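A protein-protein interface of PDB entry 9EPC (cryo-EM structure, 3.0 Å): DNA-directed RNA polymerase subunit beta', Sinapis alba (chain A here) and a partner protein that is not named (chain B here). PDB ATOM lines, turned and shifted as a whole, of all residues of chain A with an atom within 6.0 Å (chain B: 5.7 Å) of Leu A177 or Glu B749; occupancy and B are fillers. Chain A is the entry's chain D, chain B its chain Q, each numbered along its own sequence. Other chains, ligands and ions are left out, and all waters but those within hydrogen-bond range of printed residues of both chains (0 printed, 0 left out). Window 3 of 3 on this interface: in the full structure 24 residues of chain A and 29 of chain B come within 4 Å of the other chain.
Of the 10 printed residues of chain A, 5 touch a printed residue of chain B.
Hydrophobic or aromatic side chains of chain A within 4 Å of the printed part of chain B: Ile A175, Leu A177 and Phe A178.
Of the 11 printed residues of chain B, 5 touch a printed residue of chain A.
Hydrophobic or aromatic side chains of chain B within 4 Å of the printed part of chain A: Tyr B746 and Leu B750.
Among the printed residues, no Asp or Glu carboxylate lies within 4 Å of a Lys or Arg side-chain nitrogen of the other chain.
Lys A172 touches none of the printed residues of chain B.
Of the printed residues of chain B, Ile A175 touches Leu B750.
Leu A177 touches two residues of chain B.
Printed residues of chain A within 4 Å of Arg B702: Phe A178 (3.1 Å) and Thr A180 (3.3 Å).
Glu B749 touches one residue of chain A.
The nearest printed residue of chain A that does not touch Val B747 is Ser A174 (7.4 Å).
The side-chain amide nitrogen (NE2) of Gln B745 sits at hydrogen-bond distance from the side-chain hydroxyl (OH) of Tyr B746 (3.2 Å).
Among the printed residues, pairs that only touch across the chains: Leu A177 with Glu B749, Thr A180 with Arg B702, Ser A174 with Leu B750, Phe A178 with Tyr B746, Ile A175 with Leu B750, Leu A177 with Tyr B746 and Phe A178 with Val B747.
The guanidinium group (NH1) of Arg B702 is in hydrogen-bond range of the backbone carbonyl oxygen (O) of Phe A178, 3.1 Å away.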
ATOM      1  N   LYS A 172       2.377   3.781  15.554  1.00  0.00           N
ATOM      2  CA  LYS A 172       2.087   5.154  15.946  1.00  0.00           C
ATOM      3  C   LYS A 172       1.694   5.311  17.407  1.00  0.00           C
ATOM      4  O   LYS A 172       1.999   6.349  18.003  1.00  0.00           O
ATOM      5  CB  LYS A 172       0.982   5.742  15.061  1.00  0.00           C
ATOM      6  CG  LYS A 172      -0.266   4.890  14.938  1.00  0.00           C
ATOM      7  CD  LYS A 172      -1.386   5.688  14.289  1.00  0.00           C
ATOM      8  CE  LYS A 172      -2.573   4.812  13.938  1.00  0.00           C
ATOM      9  NZ  LYS A 172      -2.269   3.903  12.802  1.00  0.00           N
ATOM     10  N   TYR A 173       1.030   4.327  18.009  1.00  0.00           N
ATOM     11  CA  TYR A 173       0.604   4.457  19.396  1.00  0.00           C
ATOM     12  C   TYR A 173       1.116   3.363  20.319  1.00  0.00           C
ATOM     13  O   TYR A 173       1.155   3.578  21.532  1.00  0.00           O
ATOM     14  CB  TYR A 173      -0.932   4.505  19.493  1.00  0.00           C
ATOM     15  CG  TYR A 173      -1.668   3.502  18.627  1.00  0.00           C
ATOM     16  CD1 TYR A 173      -2.576   3.929  17.666  1.00  0.00           C
ATOM     17  CD2 TYR A 173      -1.466   2.138  18.775  1.00  0.00           C
ATOM     18  CE1 TYR A 173      -3.257   3.021  16.875  1.00  0.00           C
ATOM     19  CE2 TYR A 173      -2.140   1.224  17.987  1.00  0.00           C
ATOM     20  CZ  TYR A 173      -3.035   1.672  17.040  1.00  0.00           C
ATOM     21  OH  TYR A 173      -3.709   0.766  16.253  1.00  0.00           O
ATOM     22  N   SER A 174       1.508   2.205  19.793  1.00  0.00           N
ATOM     23  CA  SER A 174       1.909   1.093  20.650  1.00  0.00           C
ATOM     24  C   SER A 174       3.417   1.067  20.878  1.00  0.00           C
ATOM     25  O   SER A 174       3.879   1.135  22.023  1.00  0.00           O
ATOM     26  CB  SER A 174       1.433  -0.231  20.046  1.00  0.00           C
ATOM     27  OG  SER A 174       1.761  -1.316  20.894  1.00  0.00           O
ATOM     28  N   ILE A 175       4.194   0.960  19.800  1.00  0.00           N
ATOM     29  CA  ILE A 175       5.651   0.923  19.936  1.00  0.00           C
ATOM     30  C   ILE A 175       6.203   2.189  20.581  1.00  0.00           C
ATOM     31  O   ILE A 175       7.019   2.075  21.510  1.00  0.00           O
ATOM     32  CB  ILE A 175       6.301   0.620  18.575  1.00  0.00           C
ATOM     33  CG1 ILE A 175       5.941  -0.791  18.116  1.00  0.00           C
ATOM     34  CG2 ILE A 175       7.806   0.779  18.661  1.00  0.00           C
ATOM     35  CD1 ILE A 175       6.495  -1.871  19.004  1.00  0.00           C
ATOM     36  N   PRO A 176       5.830   3.403  20.154  1.00  0.00           N
ATOM     37  CA  PRO A 176       6.362   4.593  20.838  1.00  0.00           C
ATOM     38  C   PRO A 176       6.003   4.655  22.308  1.00  0.00           C
ATOM     39  O   PRO A 176       6.804   5.144  23.113  1.00  0.00           O
ATOM     40  CB  PRO A 176       5.736   5.755  20.056  1.00  0.00           C
ATOM     41  CG  PRO A 176       5.424   5.187  18.727  1.00  0.00           C
ATOM     42  CD  PRO A 176       5.000   3.781  18.997  1.00  0.00           C
ATOM     43  N   LEU A 177       4.816   4.179  22.688  1.00  0.00           N
ATOM     44  CA  LEU A 177       4.445   4.176  24.098  1.00  0.00           C
ATOM     45  C   LEU A 177       5.286   3.183  24.887  1.00  0.00           C
ATOM     46  O   LEU A 177       5.697   3.467  26.018  1.00  0.00           O
ATOM     47  CB  LEU A 177       2.960   3.859  24.247  1.00  0.00           C
ATOM     48  CG  LEU A 177       2.429   3.834  25.679  1.00  0.00           C
ATOM     49  CD1 LEU A 177       2.689   5.167  26.361  1.00  0.00           C
ATOM     50  CD2 LEU A 177       0.949   3.506  25.691  1.00  0.00           C
ATOM     51  N   PHE A 178       5.551   2.011  24.307  1.00  0.00           N
ATOM     52  CA  PHE A 178       6.296   0.977  25.015  1.00  0.00           C
ATOM     53  C   PHE A 178       7.725   1.419  25.298  1.00  0.00           C
ATOM     54  O   PHE A 178       8.238   1.230  26.407  1.00  0.00           O
ATOM     55  CB  PHE A 178       6.281  -0.315  24.198  1.00  0.00           C
ATOM     56  CG  PHE A 178       6.987  -1.462  24.857  1.00  0.00           C
ATOM     57  CD1 PHE A 178       6.332  -2.254  25.783  1.00  0.00           C
ATOM     58  CD2 PHE A 178       8.300  -1.757  24.540  1.00  0.00           C
ATOM     59  CE1 PHE A 178       6.977  -3.312  26.385  1.00  0.00           C
ATOM     60  CE2 PHE A 178       8.949  -2.814  25.140  1.00  0.00           C
ATOM     61  CZ  PHE A 178       8.286  -3.592  26.064  1.00  0.00           C
ATOM     62  N   PHE A 179       8.386   2.015  24.308  1.00  0.00           N
ATOM     63  CA  PHE A 179       9.781   2.412  24.428  1.00  0.00           C
ATOM     64  C   PHE A 179       9.954   3.871  24.822  1.00  0.00           C
ATOM     65  O   PHE A 179      11.091   4.353  24.866  1.00  0.00           O
ATOM     66  CB  PHE A 179      10.521   2.144  23.118  1.00  0.00           C
ATOM     67  CG  PHE A 179      10.700   0.690  22.811  1.00  0.00           C
ATOM     68  CD1 PHE A 179      11.671  -0.049  23.457  1.00  0.00           C
ATOM     69  CD2 PHE A 179       9.905   0.064  21.871  1.00  0.00           C
ATOM     70  CE1 PHE A 179      11.842  -1.387  23.177  1.00  0.00           C
ATOM     71  CE2 PHE A 179      10.072  -1.273  21.586  1.00  0.00           C
ATOM     72  CZ  PHE A 179      11.042  -1.999  22.240  1.00  0.00           C
ATOM     73  N   THR A 180       8.855   4.584  25.086  1.00  0.00           N
ATOM     74  CA  THR A 180       8.846   6.007  25.426  1.00  0.00           C
ATOM     75  C   THR A 180       9.282   6.847  24.233  1.00  0.00           C
ATOM     76  O   THR A 180      10.100   6.407  23.419  1.00  0.00           O
ATOM     77  CB  THR A 180       9.726   6.316  26.645  1.00  0.00           C
ATOM     78  OG1 THR A 180      11.105   6.117  26.313  1.00  0.00           O
ATOM     79  CG2 THR A 180       9.349   5.424  27.817  1.00  0.00           C
ATOM     80  N   THR A 181       8.741   8.060  24.121  1.00  0.00           N
ATOM     81  CA  THR A 181       9.004   8.893  22.951  1.00  0.00           C
ATOM     82  C   THR A 181      10.489   9.216  22.824  1.00  0.00           C
ATOM     83  O   THR A 181      11.057   9.169  21.728  1.00  0.00           O
ATOM     84  CB  THR A 181       8.176  10.175  23.030  1.00  0.00           C
ATOM     85  OG1 THR A 181       6.784   9.842  23.076  1.00  0.00           O
ATOM     86  CG2 THR A 181       8.439  11.051  21.816  1.00  0.00           C
ATOM     87  N   ARG B 702      13.943  -3.015  28.116  1.00  0.00           N
ATOM     88  CA  ARG B 702      12.506  -3.121  27.901  1.00  0.00           C
ATOM     89  C   ARG B 702      12.174  -4.293  26.987  1.00  0.00           C
ATOM     90  O   ARG B 702      11.185  -5.001  27.208  1.00  0.00           O
ATOM     91  CB  ARG B 702      11.961  -1.819  27.318  1.00  0.00           C
ATOM     92  CG  ARG B 702      12.130  -0.618  28.224  1.00  0.00           C
ATOM     93  CD  ARG B 702      11.696   0.653  27.523  1.00  0.00           C
ATOM     94  NE  ARG B 702      11.829   1.822  28.381  1.00  0.00           N
ATOM     95  CZ  ARG B 702      10.841   2.344  29.093  1.00  0.00           C
ATOM     96  NH1 ARG B 702       9.624   1.826  29.067  1.00  0.00           N
ATOM     97  NH2 ARG B 702      11.079   3.409  29.852  1.00  0.00           N
ATOM     98  N   GLN B 745       4.649  -2.373  32.639  1.00  0.00           N
ATOM     99  CA  GLN B 745       3.382  -1.653  32.599  1.00  0.00           C
ATOM    100  C   GLN B 745       2.734  -1.738  31.222  1.00  0.00           C
ATOM    101  O   GLN B 745       1.514  -1.905  31.116  1.00  0.00           O
ATOM    102  CB  GLN B 745       3.601  -0.197  33.003  1.00  0.00           C
ATOM    103  CG  GLN B 745       2.346   0.651  32.983  1.00  0.00           C
ATOM    104  CD  GLN B 745       2.608   2.079  33.414  1.00  0.00           C
ATOM    105  OE1 GLN B 745       3.698   2.409  33.880  1.00  0.00           O
ATOM    106  NE2 GLN B 745       1.607   2.938  33.261  1.00  0.00           N
ATOM    107  N   TYR B 746       3.528  -1.630  30.158  1.00  0.00           N
ATOM    108  CA  TYR B 746       3.001  -1.549  28.801  1.00  0.00           C
ATOM    109  C   TYR B 746       3.244  -2.811  27.984  1.00  0.00           C
ATOM    110  O   TYR B 746       2.959  -2.818  26.783  1.00  0.00           O
ATOM    111  CB  TYR B 746       3.599  -0.343  28.077  1.00  0.00           C
ATOM    112  CG  TYR B 746       3.366   0.971  28.781  1.00  0.00           C
ATOM    113  CD1 TYR B 746       2.163   1.649  28.647  1.00  0.00           C
ATOM    114  CD2 TYR B 746       4.352   1.538  29.575  1.00  0.00           C
ATOM    115  CE1 TYR B 746       1.947   2.852  29.290  1.00  0.00           C
ATOM    116  CE2 TYR B 746       4.145   2.741  30.220  1.00  0.00           C
ATOM    117  CZ  TYR B 746       2.942   3.393  30.073  1.00  0.00           C
ATOM    118  OH  TYR B 746       2.732   4.591  30.714  1.00  0.00           O
ATOM    119  N   VAL B 747       3.764  -3.878  28.595  1.00  0.00           N
ATOM    120  CA  VAL B 747       4.007  -5.103  27.839  1.00  0.00           C
ATOM    121  C   VAL B 747       2.690  -5.729  27.396  1.00  0.00           C
ATOM    122  O   VAL B 747       2.594  -6.295  26.301  1.00  0.00           O
ATOM    123  CB  VAL B 747       4.861  -6.085  28.663  1.00  0.00           C
ATOM    124  CG1 VAL B 747       4.193  -6.401  29.989  1.00  0.00           C
ATOM    125  CG2 VAL B 747       5.119  -7.358  27.874  1.00  0.00           C
ATOM    126  N   ASP B 748       1.655  -5.631  28.232  1.00  0.00           N
ATOM    127  CA  ASP B 748       0.362  -6.211  27.881  1.00  0.00           C
ATOM    128  C   ASP B 748      -0.235  -5.529  26.658  1.00  0.00           C
ATOM    129  O   ASP B 748      -0.833  -6.188  25.800  1.00  0.00           O
ATOM    130  CB  ASP B 748      -0.592  -6.117  29.069  1.00  0.00           C
ATOM    131  CG  ASP B 748      -0.766  -4.696  29.561  1.00  0.00           C
ATOM    132  OD1 ASP B 748       0.170  -3.888  29.384  1.00  0.00           O
ATOM    133  OD2 ASP B 748      -1.837  -4.387  30.123  1.00  0.00           O
ATOM    134  N   GLU B 749      -0.086  -4.205  26.561  1.00  0.00           N
ATOM    135  CA  GLU B 749      -0.598  -3.488  25.399  1.00  0.00           C
ATOM    136  C   GLU B 749       0.098  -3.942  24.125  1.00  0.00           C
ATOM    137  O   GLU B 749      -0.515  -3.983  23.052  1.00  0.00           O
ATOM    138  CB  GLU B 749      -0.432  -1.983  25.590  1.00  0.00           C
ATOM    139  CG  GLU B 749      -1.160  -1.426  26.797  1.00  0.00           C
ATOM    140  CD  GLU B 749      -1.081   0.085  26.873  1.00  0.00           C
ATOM    141  OE1 GLU B 749      -0.626   0.703  25.888  1.00  0.00           O
ATOM    142  OE2 GLU B 749      -1.471   0.653  27.914  1.00  0.00           O
ATOM    143  N   LEU B 750       1.386  -4.274  24.220  1.00  0.00           N
ATOM    144  CA  LEU B 750       2.099  -4.774  23.052  1.00  0.00           C
ATOM    145  C   LEU B 750       1.527  -6.109  22.593  1.00  0.00           C
ATOM    146  O   LEU B 750       1.344  -6.334  21.391  1.00  0.00           O
ATOM    147  CB  LEU B 750       3.587  -4.902  23.368  1.00  0.00           C
ATOM    148  CG  LEU B 750       4.534  -4.795  22.175  1.00  0.00           C
ATOM    149  CD1 LEU B 750       4.269  -3.508  21.424  1.00  0.00           C
ATOM    150  CD2 LEU B 750       5.973  -4.850  22.643  1.00  0.00           C
ATOM    151  N   HIS B 751       1.230  -7.005  23.535  1.00  0.00           N
ATOM    152  CA  HIS B 751       0.669  -8.300  23.164  1.00  0.00           C
ATOM    153  C   HIS B 751      -0.764  -8.165  22.666  1.00  0.00           C
ATOM    154  O   HIS B 751      -1.173  -8.873  21.740  1.00  0.00           O
ATOM    155  CB  HIS B 751       0.741  -9.262  24.348  1.00  0.00           C
ATOM    156  CG  HIS B 751       2.125  -9.739  24.651  1.00  0.00           C
ATOM    157  ND1 HIS B 751       2.709 -10.794  23.984  1.00  0.00           N
ATOM    158  CD2 HIS B 751       3.043  -9.303  25.544  1.00  0.00           C
ATOM    159  CE1 HIS B 751       3.927 -10.990  24.456  1.00  0.00           C
ATOM    160  NE2 HIS B 751       4.155 -10.098  25.403  1.00  0.00           N
ATOM    161  N   GLN B 752      -1.543  -7.261  23.266  1.00  0.00           N
ATOM    162  CA  GLN B 752      -2.916  -7.063  22.817  1.00  0.00           C
ATOM    163  C   GLN B 752      -2.979  -6.429  21.435  1.00  0.00           C
ATOM    164  O   GLN B 752      -4.040  -6.450  20.805  1.00  0.00           O
ATOM    165  CB  GLN B 752      -3.686  -6.201  23.820  1.00  0.00           C
ATOM    166  CG  GLN B 752      -3.517  -4.708  23.613  1.00  0.00           C
ATOM    167  CD  GLN B 752      -4.125  -3.889  24.733  1.00  0.00           C
ATOM    168  OE1 GLN B 752      -4.621  -4.436  25.717  1.00  0.00           O
ATOM    169  NE2 GLN B 752      -4.088  -2.571  24.589  1.00  0.00           N
ATOM    170  N   ALA B 753      -1.873  -5.868  20.955  1.00  0.00           N
ATOM    171  CA  ALA B 753      -1.791  -5.303  19.617  1.00  0.00           C
ATOM    172  C   ALA B 753      -1.311  -6.314  18.585  1.00  0.00           C
ATOM    173  O   ALA B 753      -1.098  -5.945  17.425  1.00  0.00           O
ATOM    174  CB  ALA B 753      -0.872  -4.081  19.615  1.00  0.00           C
ATOM    175  N   GLY B 754      -1.134  -7.572  18.976  1.00  0.00           N
ATOM    176  CA  GLY B 754      -0.699  -8.602  18.060  1.00  0.00           C
ATOM    177  C   GLY B 754       0.795  -8.710  17.866  1.00  0.00           C
ATOM    178  O   GLY B 754       1.232  -9.428  16.959  1.00  0.00           O
